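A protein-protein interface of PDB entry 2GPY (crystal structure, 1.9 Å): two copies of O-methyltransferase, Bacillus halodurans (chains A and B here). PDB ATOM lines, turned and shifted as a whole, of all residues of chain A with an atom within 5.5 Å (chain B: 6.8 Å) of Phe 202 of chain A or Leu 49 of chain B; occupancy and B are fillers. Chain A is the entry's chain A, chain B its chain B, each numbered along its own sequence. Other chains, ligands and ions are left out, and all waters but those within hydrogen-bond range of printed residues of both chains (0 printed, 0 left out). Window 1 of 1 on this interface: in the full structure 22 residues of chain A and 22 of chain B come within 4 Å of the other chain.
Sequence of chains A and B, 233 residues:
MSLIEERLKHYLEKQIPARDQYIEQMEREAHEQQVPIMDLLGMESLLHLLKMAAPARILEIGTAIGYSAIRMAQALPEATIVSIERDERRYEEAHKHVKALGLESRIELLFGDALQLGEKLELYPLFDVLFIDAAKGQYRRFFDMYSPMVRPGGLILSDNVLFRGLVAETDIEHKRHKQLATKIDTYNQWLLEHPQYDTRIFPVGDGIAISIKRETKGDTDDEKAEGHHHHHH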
ATOM      1  N   LEU A  49      -1.774  -5.793 -17.053  1.00  0.00           N
ATOM      2  CA  LEU A  49      -2.664  -4.623 -16.993  1.00  0.00           C
ATOM      3  C   LEU A  49      -4.055  -5.004 -17.514  1.00  0.00           C
ATOM      4  O   LEU A  49      -5.087  -4.609 -16.953  1.00  0.00           O
ATOM      5  CB  LEU A  49      -2.103  -3.485 -17.845  1.00  0.00           C
ATOM      6  CG  LEU A  49      -0.804  -2.791 -17.431  1.00  0.00           C
ATOM      7  CD1 LEU A  49      -0.366  -1.857 -18.588  1.00  0.00           C
ATOM      8  CD2 LEU A  49      -0.972  -2.005 -16.153  1.00  0.00           C
ATOM      9  N   MET A  52      -6.067  -6.998 -15.051  1.00  0.00           N
ATOM     10  CA  MET A  52      -6.589  -6.124 -13.985  1.00  0.00           C
ATOM     11  C   MET A  52      -7.865  -5.391 -14.392  1.00  0.00           C
ATOM     12  O   MET A  52      -8.720  -5.091 -13.550  1.00  0.00           O
ATOM     13  CB  MET A  52      -5.555  -5.062 -13.600  1.00  0.00           C
ATOM     14  CG  MET A  52      -4.198  -5.569 -13.201  1.00  0.00           C
ATOM     15  SD  MET A  52      -2.956  -4.088 -12.989  1.00  0.00           S
ATOM     16  CE  MET A  52      -3.812  -3.181 -11.370  1.00  0.00           C
ATOM     17  N   ARG A 200      -2.357   8.530 -18.589  1.00  0.00           N
ATOM     18  CA  ARG A 200      -1.027   8.449 -17.986  1.00  0.00           C
ATOM     19  C   ARG A 200      -0.141   7.512 -18.796  1.00  0.00           C
ATOM     20  O   ARG A 200      -0.600   6.485 -19.298  1.00  0.00           O
ATOM     21  CB  ARG A 200      -1.108   7.992 -16.530  1.00  0.00           C
ATOM     22  CG  ARG A 200       0.196   8.113 -15.786  1.00  0.00           C
ATOM     23  CD  ARG A 200       0.008   8.054 -14.267  1.00  0.00           C
ATOM     24  NE  ARG A 200       1.275   8.229 -13.568  1.00  0.00           N
ATOM     25  CZ  ARG A 200       1.832   9.409 -13.295  1.00  0.00           C
ATOM     26  NH1 ARG A 200       1.230  10.541 -13.651  1.00  0.00           N
ATOM     27  NH2 ARG A 200       2.997   9.457 -12.659  1.00  0.00           N
ATOM     28  N   ILE A 201       1.130   7.881 -18.909  1.00  0.00           N
ATOM     29  CA  ILE A 201       2.104   7.050 -19.587  1.00  0.00           C
ATOM     30  C   ILE A 201       2.792   6.137 -18.582  1.00  0.00           C
ATOM     31  O   ILE A 201       3.225   6.581 -17.498  1.00  0.00           O
ATOM     32  CB  ILE A 201       3.122   7.891 -20.377  1.00  0.00           C
ATOM     33  CG1 ILE A 201       2.408   8.646 -21.514  1.00  0.00           C
ATOM     34  CG2 ILE A 201       4.245   7.001 -20.943  1.00  0.00           C
ATOM     35  CD1 ILE A 201       3.385   9.366 -22.411  1.00  0.00           C
ATOM     36  N   PHE A 202       2.888   4.861 -18.956  1.00  0.00           N
ATOM     37  CA  PHE A 202       3.551   3.862 -18.146  1.00  0.00           C
ATOM     38  C   PHE A 202       4.820   3.326 -18.791  1.00  0.00           C
ATOM     39  O   PHE A 202       4.892   3.219 -20.015  1.00  0.00           O
ATOM     40  CB  PHE A 202       2.569   2.742 -17.840  1.00  0.00           C
ATOM     41  CG  PHE A 202       1.714   3.029 -16.659  1.00  0.00           C
ATOM     42  CD1 PHE A 202       0.649   3.929 -16.758  1.00  0.00           C
ATOM     43  CD2 PHE A 202       1.990   2.449 -15.436  1.00  0.00           C
ATOM     44  CE1 PHE A 202      -0.153   4.209 -15.636  1.00  0.00           C
ATOM     45  CE2 PHE A 202       1.200   2.724 -14.315  1.00  0.00           C
ATOM     46  CZ  PHE A 202       0.131   3.610 -14.430  1.00  0.00           C
ATOM     47  N   PRO A 203       5.842   3.023 -17.974  1.00  0.00           N
ATOM     48  CA  PRO A 203       7.090   2.535 -18.556  1.00  0.00           C
ATOM     49  C   PRO A 203       7.022   1.068 -18.979  1.00  0.00           C
ATOM     50  O   PRO A 203       7.617   0.203 -18.337  1.00  0.00           O
ATOM     51  CB  PRO A 203       8.129   2.760 -17.448  1.00  0.00           C
ATOM     52  CG  PRO A 203       7.371   3.293 -16.255  1.00  0.00           C
ATOM     53  CD  PRO A 203       5.916   3.115 -16.506  1.00  0.00           C
ATOM     54  N   VAL A 204       6.288   0.804 -20.056  1.00  0.00           N
ATOM     55  CA  VAL A 204       6.285  -0.502 -20.708  1.00  0.00           C
ATOM     56  C   VAL A 204       6.884  -0.252 -22.083  1.00  0.00           C
ATOM     57  O   VAL A 204       6.572   0.758 -22.716  1.00  0.00           O
ATOM     58  CB  VAL A 204       4.851  -1.072 -20.839  1.00  0.00           C
ATOM     59  CG1 VAL A 204       4.878  -2.455 -21.457  1.00  0.00           C
ATOM     60  CG2 VAL A 204       4.154  -1.120 -19.470  1.00  0.00           C
ATOM     61  N   GLY A 207       7.176   3.209 -23.728  1.00  0.00           N
ATOM     62  CA  GLY A 207       6.193   4.083 -23.117  1.00  0.00           C
ATOM     63  C   GLY A 207       4.837   3.792 -23.731  1.00  0.00           C
ATOM     64  O   GLY A 207       4.673   3.879 -24.960  1.00  0.00           O
ATOM     65  N   ILE A 208       3.881   3.425 -22.885  1.00  0.00           N
ATOM     66  CA  ILE A 208       2.515   3.182 -23.325  1.00  0.00           C
ATOM     67  C   ILE A 208       1.560   4.120 -22.588  1.00  0.00           C
ATOM     68  O   ILE A 208       1.628   4.247 -21.366  1.00  0.00           O
ATOM     69  CB  ILE A 208       2.108   1.676 -23.182  1.00  0.00           C
ATOM     70  CG1 ILE A 208       0.756   1.418 -23.858  1.00  0.00           C
ATOM     71  CG2 ILE A 208       2.101   1.222 -21.709  1.00  0.00           C
ATOM     72  CD1 ILE A 208       0.486  -0.036 -24.160  1.00  0.00           C
ATOM     73  N   ALA A 209       0.700   4.796 -23.340  1.00  0.00           N
ATOM     74  CA  ALA A 209      -0.309   5.684 -22.764  1.00  0.00           C
ATOM     75  C   ALA A 209      -1.483   4.803 -22.330  1.00  0.00           C
ATOM     76  O   ALA A 209      -1.947   3.959 -23.080  1.00  0.00           O
ATOM     77  CB  ALA A 209      -0.761   6.715 -23.766  1.00  0.00           C
ATOM     78  N   ILE A 210      -1.923   4.960 -21.098  1.00  0.00           N
ATOM     79  CA  ILE A 210      -3.135   4.312 -20.658  1.00  0.00           C
ATOM     80  C   ILE A 210      -4.190   5.391 -20.502  1.00  0.00           C
ATOM     81  O   ILE A 210      -4.102   6.208 -19.597  1.00  0.00           O
ATOM     82  CB  ILE A 210      -2.939   3.583 -19.310  1.00  0.00           C
ATOM     83  CG1 ILE A 210      -1.854   2.507 -19.463  1.00  0.00           C
ATOM     84  CG2 ILE A 210      -4.252   2.980 -18.871  1.00  0.00           C
ATOM     85  CD1 ILE A 210      -1.468   1.814 -18.151  1.00  0.00           C
ATOM     86  N   LEU B   8      12.964   9.880 -22.119  1.00  0.00           N
ATOM     87  CA  LEU B   8      11.773   9.067 -21.708  1.00  0.00           C
ATOM     88  C   LEU B   8      11.649   8.963 -20.186  1.00  0.00           C
ATOM     89  O   LEU B   8      10.638   9.373 -19.613  1.00  0.00           O
ATOM     90  CB  LEU B   8      11.809   7.663 -22.345  1.00  0.00           C
ATOM     91  CG  LEU B   8      10.866   6.556 -21.826  1.00  0.00           C
ATOM     92  CD1 LEU B   8       9.388   6.949 -21.905  1.00  0.00           C
ATOM     93  CD2 LEU B   8      11.111   5.227 -22.552  1.00  0.00           C
ATOM     94  N   LEU B  12       9.016  10.786 -17.634  1.00  0.00           N
ATOM     95  CA  LEU B  12       8.241  10.067 -16.619  1.00  0.00           C
ATOM     96  C   LEU B  12       8.503  10.612 -15.208  1.00  0.00           C
ATOM     97  O   LEU B  12       7.588  10.641 -14.383  1.00  0.00           O
ATOM     98  CB  LEU B  12       8.525   8.555 -16.675  1.00  0.00           C
ATOM     99  CG  LEU B  12       8.175   7.831 -17.986  1.00  0.00           C
ATOM    100  CD1 LEU B  12       8.938   6.513 -18.134  1.00  0.00           C
ATOM    101  CD2 LEU B  12       6.666   7.619 -18.141  1.00  0.00           C
ATOM    102  N   GLN B  15       6.078  13.551 -14.455  1.00  0.00           N
ATOM    103  CA  GLN B  15       4.652  13.350 -14.729  1.00  0.00           C
ATOM    104  C   GLN B  15       3.776  13.455 -13.466  1.00  0.00           C
ATOM    105  O   GLN B  15       3.280  12.442 -12.953  1.00  0.00           O
ATOM    106  CB  GLN B  15       4.427  12.009 -15.448  1.00  0.00           C
ATOM    107  CG  GLN B  15       3.096  11.928 -16.202  1.00  0.00           C
ATOM    108  CD  GLN B  15       2.830  10.568 -16.851  1.00  0.00           C
ATOM    109  OE1 GLN B  15       1.957  10.453 -17.708  1.00  0.00           O
ATOM    110  NE2 GLN B  15       3.565   9.540 -16.432  1.00  0.00           N
ATOM    111  N   GLY B  42       4.974   6.775  -7.483  1.00  0.00           N
ATOM    112  CA  GLY B  42       4.271   5.506  -7.233  1.00  0.00           C
ATOM    113  C   GLY B  42       2.783   5.717  -6.974  1.00  0.00           C
ATOM    114  O   GLY B  42       1.934   4.923  -7.411  1.00  0.00           O
ATOM    115  N   GLU B  44       0.827   8.237  -7.958  1.00  0.00           N
ATOM    116  CA  GLU B  44       0.091   8.639  -9.156  1.00  0.00           C
ATOM    117  C   GLU B  44      -0.166   7.426 -10.056  1.00  0.00           C
ATOM    118  O   GLU B  44      -1.256   7.267 -10.626  1.00  0.00           O
ATOM    119  CB  GLU B  44       0.837   9.734  -9.919  1.00  0.00           C
ATOM    120  CG  GLU B  44       0.901  11.062  -9.139  1.00  0.00           C
ATOM    121  CD  GLU B  44      -0.476  11.743  -8.968  1.00  0.00           C
ATOM    122  OE1 GLU B  44      -1.381  11.521  -9.800  1.00  0.00           O
ATOM    123  OE2 GLU B  44      -0.642  12.509  -7.998  1.00  0.00           O
ATOM    124  N   SER B  45       0.855   6.590 -10.193  1.00  0.00           N
ATOM    125  CA  SER B  45       0.706   5.352 -10.973  1.00  0.00           C
ATOM    126  C   SER B  45      -0.292   4.409 -10.366  1.00  0.00           C
ATOM    127  O   SER B  45      -1.140   3.856 -11.091  1.00  0.00           O
ATOM    128  CB  SER B  45       2.058   4.661 -11.161  1.00  0.00           C
ATOM    129  OG  SER B  45       2.783   5.389 -12.117  1.00  0.00           O
ATOM    130  N   LEU B  46      -0.229   4.228  -9.050  1.00  0.00           N
ATOM    131  CA  LEU B  46      -1.186   3.368  -8.371  1.00  0.00           C
ATOM    132  C   LEU B  46      -2.612   3.849  -8.569  1.00  0.00           C
ATOM    133  O   LEU B  46      -3.511   3.046  -8.818  1.00  0.00           O
ATOM    134  CB  LEU B  46      -0.899   3.243  -6.867  1.00  0.00           C
ATOM    135  CG  LEU B  46      -1.714   2.142  -6.180  1.00  0.00           C
ATOM    136  CD1 LEU B  46      -1.246   0.774  -6.724  1.00  0.00           C
ATOM    137  CD2 LEU B  46      -1.634   2.187  -4.680  1.00  0.00           C
ATOM    138  N   LEU B  47      -2.836   5.149  -8.417  1.00  0.00           N
ATOM    139  CA  LEU B  47      -4.202   5.666  -8.532  1.00  0.00           C
ATOM    140  C   LEU B  47      -4.723   5.434  -9.954  1.00  0.00           C
ATOM    141  O   LEU B  47      -5.901   5.094 -10.182  1.00  0.00           O
ATOM    142  CB  LEU B  47      -4.194   7.165  -8.221  1.00  0.00           C
ATOM    143  CG  LEU B  47      -3.880   7.470  -6.750  1.00  0.00           C
ATOM    144  CD1 LEU B  47      -3.785   8.976  -6.651  1.00  0.00           C
ATOM    145  CD2 LEU B  47      -4.984   6.908  -5.809  1.00  0.00           C
ATOM    146  N   HIS B  48      -3.851   5.615 -10.932  1.00  0.00           N
ATOM    147  CA  HIS B  48      -4.272   5.387 -12.330  1.00  0.00           C
ATOM    148  C   HIS B  48      -4.636   3.911 -12.586  1.00  0.00           C
ATOM    149  O   HIS B  48      -5.628   3.594 -13.288  1.00  0.00           O
ATOM    150  CB  HIS B  48      -3.193   5.852 -13.291  1.00  0.00           C
ATOM    151  CG  HIS B  48      -3.715   6.158 -14.667  1.00  0.00           C
ATOM    152  ND1 HIS B  48      -4.513   7.245 -14.918  1.00  0.00           N
ATOM    153  CD2 HIS B  48      -3.584   5.505 -15.844  1.00  0.00           C
ATOM    154  CE1 HIS B  48      -4.848   7.262 -16.199  1.00  0.00           C
ATOM    155  NE2 HIS B  48      -4.287   6.223 -16.785  1.00  0.00           N
ATOM    156  N   LEU B  49      -3.830   3.005 -12.051  1.00  0.00           N
ATOM    157  CA  LEU B  49      -4.108   1.570 -12.185  1.00  0.00           C
ATOM    158  C   LEU B  49      -5.419   1.211 -11.473  1.00  0.00           C
ATOM    159  O   LEU B  49      -6.221   0.413 -11.973  1.00  0.00           O
ATOM    160  CB  LEU B  49      -2.957   0.750 -11.622  1.00  0.00           C
ATOM    161  CG  LEU B  49      -1.600   0.860 -12.353  1.00  0.00           C
ATOM    162  CD1 LEU B  49      -0.540   0.205 -11.475  1.00  0.00           C
ATOM    163  CD2 LEU B  49      -1.618   0.262 -13.735  1.00  0.00           C
ATOM    164  N   LEU B  50      -5.653   1.811 -10.316  1.00  0.00           N
ATOM    165  CA  LEU B  50      -6.929   1.617  -9.632  1.00  0.00           C
ATOM    166  C   LEU B  50      -8.102   2.103 -10.478  1.00  0.00           C
ATOM    167  O   LEU B  50      -9.121   1.421 -10.553  1.00  0.00           O
ATOM    168  CB  LEU B  50      -6.940   2.299  -8.259  1.00  0.00           C
ATOM    169  CG  LEU B  50      -6.083   1.680  -7.156  1.00  0.00           C
ATOM    170  CD1 LEU B  50      -5.901   2.671  -6.000  1.00  0.00           C
ATOM    171  CD2 LEU B  50      -6.678   0.368  -6.647  1.00  0.00           C
ATOM    172  N   LYS B  51      -7.995   3.289 -11.091  1.00  0.00           N
ATOM    173  CA  LYS B  51      -9.082   3.808 -11.902  1.00  0.00           C
ATOM    174  C   LYS B  51      -9.385   2.850 -13.036  1.00  0.00           C
ATOM    175  O   LYS B  51     -10.554   2.689 -13.444  1.00  0.00           O
ATOM    176  CB  LYS B  51      -8.760   5.194 -12.487  1.00  0.00           C
ATOM    177  CG  LYS B  51      -8.730   6.330 -11.453  1.00  0.00           C
ATOM    178  CD  LYS B  51      -8.445   7.621 -12.188  1.00  0.00           C
ATOM    179  CE  LYS B  51      -7.659   8.577 -11.347  1.00  0.00           C
ATOM    180  NZ  LYS B  51      -7.529   9.896 -12.116  1.00  0.00           N
ATOM    181  N   MET B  52      -8.327   2.224 -13.547  1.00  0.00           N
ATOM    182  CA  MET B  52      -8.439   1.294 -14.638  1.00  0.00           C
ATOM    183  C   MET B  52      -9.209   0.047 -14.201  1.00  0.00           C
ATOM    184  O   MET B  52     -10.019  -0.490 -14.971  1.00  0.00           O
ATOM    185  CB  MET B  52      -7.022   0.912 -15.084  1.00  0.00           C
ATOM    186  CG  MET B  52      -6.956   0.294 -16.353  1.00  0.00           C
ATOM    187  SD  MET B  52      -5.124  -0.257 -16.745  1.00  0.00           S
ATOM    188  CE  MET B  52      -4.210   0.778 -15.779  1.00  0.00           C
ATOM    189  N   ALA B  53      -8.906  -0.437 -12.997  1.00  0.00           N
ATOM    190  CA  ALA B  53      -9.581  -1.597 -12.413  1.00  0.00           C
ATOM    191  C   ALA B  53     -10.971  -1.304 -11.844  1.00  0.00           C
ATOM    192  O   ALA B  53     -11.753  -2.232 -11.694  1.00  0.00           O
ATOM    193  CB  ALA B  53      -8.713  -2.230 -11.357  1.00  0.00           C
ATOM    194  N   ALA B  54     -11.268  -0.039 -11.512  1.00  0.00           N
ATOM    195  CA  ALA B  54     -12.615   0.402 -11.057  1.00  0.00           C
ATOM    196  C   ALA B  54     -13.164  -0.381  -9.841  1.00  0.00           C
ATOM    197  O   ALA B  54     -14.309  -0.877  -9.869  1.00  0.00           O
ATOM    198  CB  ALA B  54     -13.639   0.403 -12.227  1.00  0.00           C
ATOM    199  N   PRO B  55     -12.366  -0.495  -8.771  1.00  0.00           N
ATOM    200  CA  PRO B  55     -12.839  -1.286  -7.622  1.00  0.00           C
ATOM    201  C   PRO B  55     -13.913  -0.518  -6.847  1.00  0.00           C
ATOM    202  O   PRO B  55     -13.891   0.709  -6.848  1.00  0.00           O
ATOM    203  CB  PRO B  55     -11.578  -1.469  -6.791  1.00  0.00           C
ATOM    204  CG  PRO B  55     -10.726  -0.244  -7.094  1.00  0.00           C
ATOM    205  CD  PRO B  55     -11.016   0.067  -8.546  1.00  0.00           C
ATOM    206  N   LEU B 155      -7.524  -7.743  -6.402  1.00  0.00           N
ATOM    207  CA  LEU B 155      -6.108  -7.401  -6.407  1.00  0.00           C
ATOM    208  C   LEU B 155      -5.567  -7.279  -5.006  1.00  0.00           C
ATOM    209  O   LEU B 155      -6.188  -6.672  -4.143  1.00  0.00           O
ATOM    210  CB  LEU B 155      -5.891  -6.033  -7.062  1.00  0.00           C
ATOM    211  CG  LEU B 155      -6.503  -5.899  -8.460  1.00  0.00           C
ATOM    212  CD1 LEU B 155      -6.361  -4.466  -9.024  1.00  0.00           C
ATOM    213  CD2 LEU B 155      -5.896  -6.937  -9.424  1.00  0.00           C
ATOM    214  N   LEU B 157      -2.299  -5.337  -3.711  1.00  0.00           N
ATOM    215  CA  LEU B 157      -1.243  -4.418  -4.134  1.00  0.00           C
ATOM    216  C   LEU B 157      -0.242  -4.287  -2.998  1.00  0.00           C
ATOM    217  O   LEU B 157      -0.629  -3.992  -1.846  1.00  0.00           O
ATOM    218  CB  LEU B 157      -1.841  -3.041  -4.450  1.00  0.00           C
ATOM    219  CG  LEU B 157      -3.000  -3.044  -5.435  1.00  0.00           C
ATOM    220  CD1 LEU B 157      -3.628  -1.635  -5.460  1.00  0.00           C
ATOM    221  CD2 LEU B 157      -2.529  -3.492  -6.792  1.00  0.00           C
ATOM    222  N   PHE B 202       5.710  -4.207 -10.824  1.00  0.00           N
ATOM    223  CA  PHE B 202       5.808  -3.071 -11.752  1.00  0.00           C
ATOM    224  C   PHE B 202       6.864  -2.084 -11.262  1.00  0.00           C
ATOM    225  O   PHE B 202       6.838  -1.703 -10.100  1.00  0.00           O
ATOM    226  CB  PHE B 202       4.460  -2.347 -11.883  1.00  0.00           C
ATOM    227  CG  PHE B 202       3.472  -3.026 -12.813  1.00  0.00           C
ATOM    228  CD1 PHE B 202       3.816  -4.182 -13.520  1.00  0.00           C
ATOM    229  CD2 PHE B 202       2.210  -2.478 -13.017  1.00  0.00           C
ATOM    230  CE1 PHE B 202       2.905  -4.808 -14.376  1.00  0.00           C
ATOM    231  CE2 PHE B 202       1.290  -3.090 -13.875  1.00  0.00           C
ATOM    232  CZ  PHE B 202       1.646  -4.259 -14.560  1.00  0.00           C
ATOM    233  N   VAL B 204       7.554   1.027 -10.836  1.00  0.00           N
ATOM    234  CA  VAL B 204       7.099   2.391 -10.640  1.00  0.00           C
ATOM    235  C   VAL B 204       7.189   2.720  -9.148  1.00  0.00           C
ATOM    236  O   VAL B 204       6.912   1.864  -8.301  1.00  0.00           O
ATOM    237  CB  VAL B 204       5.667   2.580 -11.168  1.00  0.00           C
ATOM    238  CG1 VAL B 204       4.678   1.609 -10.492  1.00  0.00           C
ATOM    239  CG2 VAL B 204       5.240   3.998 -11.018  1.00  0.00           C
ATOM    240  N   ILE B 208       5.813  -1.830  -7.039  1.00  0.00           N
ATOM    241  CA  ILE B 208       4.480  -2.219  -6.626  1.00  0.00           C
ATOM    242  C   ILE B 208       4.221  -3.607  -7.174  1.00  0.00           C
ATOM    243  O   ILE B 208       4.304  -3.813  -8.389  1.00  0.00           O
ATOM    244  CB  ILE B 208       3.417  -1.278  -7.168  1.00  0.00           C
ATOM    245  CG1 ILE B 208       3.699   0.187  -6.746  1.00  0.00           C
ATOM    246  CG2 ILE B 208       2.013  -1.738  -6.662  1.00  0.00           C
ATOM    247  CD1 ILE B 208       2.758   1.180  -7.428  1.00  0.00           C
ATOM    248  N   ILE B 210       1.548  -6.401  -8.033  1.00  0.00           N
ATOM    249  CA  ILE B 210       0.105  -6.511  -8.276  1.00  0.00           C
ATOM    250  C   ILE B 210      -0.205  -7.985  -8.392  1.00  0.00           C
ATOM    251  O   ILE B 210       0.196  -8.649  -9.353  1.00  0.00           O
ATOM    252  CB  ILE B 210      -0.303  -5.789  -9.550  1.00  0.00           C
ATOM    253  CG1 ILE B 210       0.100  -4.311  -9.438  1.00  0.00           C
ATOM    254  CG2 ILE B 210      -1.804  -5.880  -9.762  1.00  0.00           C
ATOM    255  CD1 ILE B 210       0.701  -3.852 -10.687  1.00  0.00           C
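The backbone NH (N) of Phe 202 of chain A sits at hydrogen-bond distance from the backbone carbonyl oxygen (O) of Ile 208 of chain A.
The backbone NH (N) of Phe 202 of chain B lies within hydrogen-bond range of the backbone carbonyl oxygen (O) of Ile 208 of chain B.
N of Ile 210 of chain A sits at hydrogen-bond distance from O of Arg 200 of chain A, at 2.7 Å.
Of the 11 printed residues of chain A, 7 touch a printed residue of chain B.
Printed residues of chain A that touch a printed residue of chain B: Leu 49, Met 52, Arg 200, Ile 201, Phe 202, Pro 203 and Ile 210.
Hydrophobic or aromatic side chains of chain A that line the printed part of chain B: Leu 49, Met 52, Ile 201, Phe 202, Pro 203 and Ile 210.
Of the 22 printed residues of chain B, 11 touch a printed residue of chain A.
Printed residues of chain B that touch a printed residue of chain A: Leu 12, Gln 15, Glu 44, Ser 45, His 48, Leu 49, Met 52, Ala 53, Leu 155, Phe 202 and Ile 210.
Among the printed residues, no Asp or Glu carboxylate lies within 4 Å of a Lys or Arg side-chain nitrogen of the other chain.
Among the printed residues, merely in contact across the chains: Leu 49 of chain A with Leu 49 of chain B, Leu 49 of chain A with Phe 202 of chain B, Arg 200 of chain A with Glu 44 of chain B, Arg 200 of chain A with His 48 of chain B, Arg 200 of chain A with Ser 45 of chain B, Phe 202 of chain A with Ser 45 of chain B, Met 52 of chain A with Ala 53 of chain B, Ile 201 of chain A with Leu 12 of chain B, Phe 202 of chain A with His 48 of chain B, Met 52 of chain A with Leu 155 of chain B, Met 52 of chain A with Ile 210 of chain B, Ile 210 of chain A with Met 52 of chain B, Phe 202 of chain A with Leu 49 of chain B and Pro 203 of chain A with Leu 12 of chain B.
Of the printed residues of chain B, Ile 201 of chain A touches Leu 12 (3.7 Å) and Gln 15 (3.0 Å).
Phe 202 of chain A touches just these residues of chain B: Ser 45, His 48 and Leu 49.
Printed residues of chain A within 4 Å of Gln 15 of chain B: Arg 200 (2.9 Å) and Ile 201 (3.0 Å).
Of the printed residues of chain A, Ser 45 of chain B touches Arg 200 and Phe 202.
Of chain A, only Leu 49 (3.4 Å) and Phe 202 (3.8 Å) come within 4 Å of Leu 49 of chain B.
Of the printed residues of chain A, Phe 202 of chain B touches Leu 49 (3.4 Å).
Ile 208 of chain B touches none of the printed residues of chain A.
The nearest residue of chain B that does not touch Phe 202 of chain A is Leu 12 of chain B (4.7 Å).
Leu 49 of chain B touches its own counterpart, Leu 49 of chain A.
Leu 49 of chain A touches Phe 202 of chain B, and with the chains exchanged Phe 202 of chain A touches Leu 49 of chain B.
Met 52 of chain A touches Ile 210 of chain B, and with the chains exchanged Ile 210 of chain A touches Met 52 of chain B.
Of the 17 pairs that touch across the chains among the printed residues, 5 have their exchanged pair printed and touching as well.
The guanidinium group (NH1) of Arg 200 of chain A is in hydrogen-bond range of the backbone carbonyl oxygen (O) of Gln 15 of chain B (2.9 Å).
The backbone carbonyl oxygen (O) of Ile 210 of chain A sits at hydrogen-bond distance from a ring nitrogen (NE2) of His 48 of chain B.
N of Ile 201 of chain A sits at hydrogen-bond distance from OE1 of Gln 15 of chain B, 3.0 Å away.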
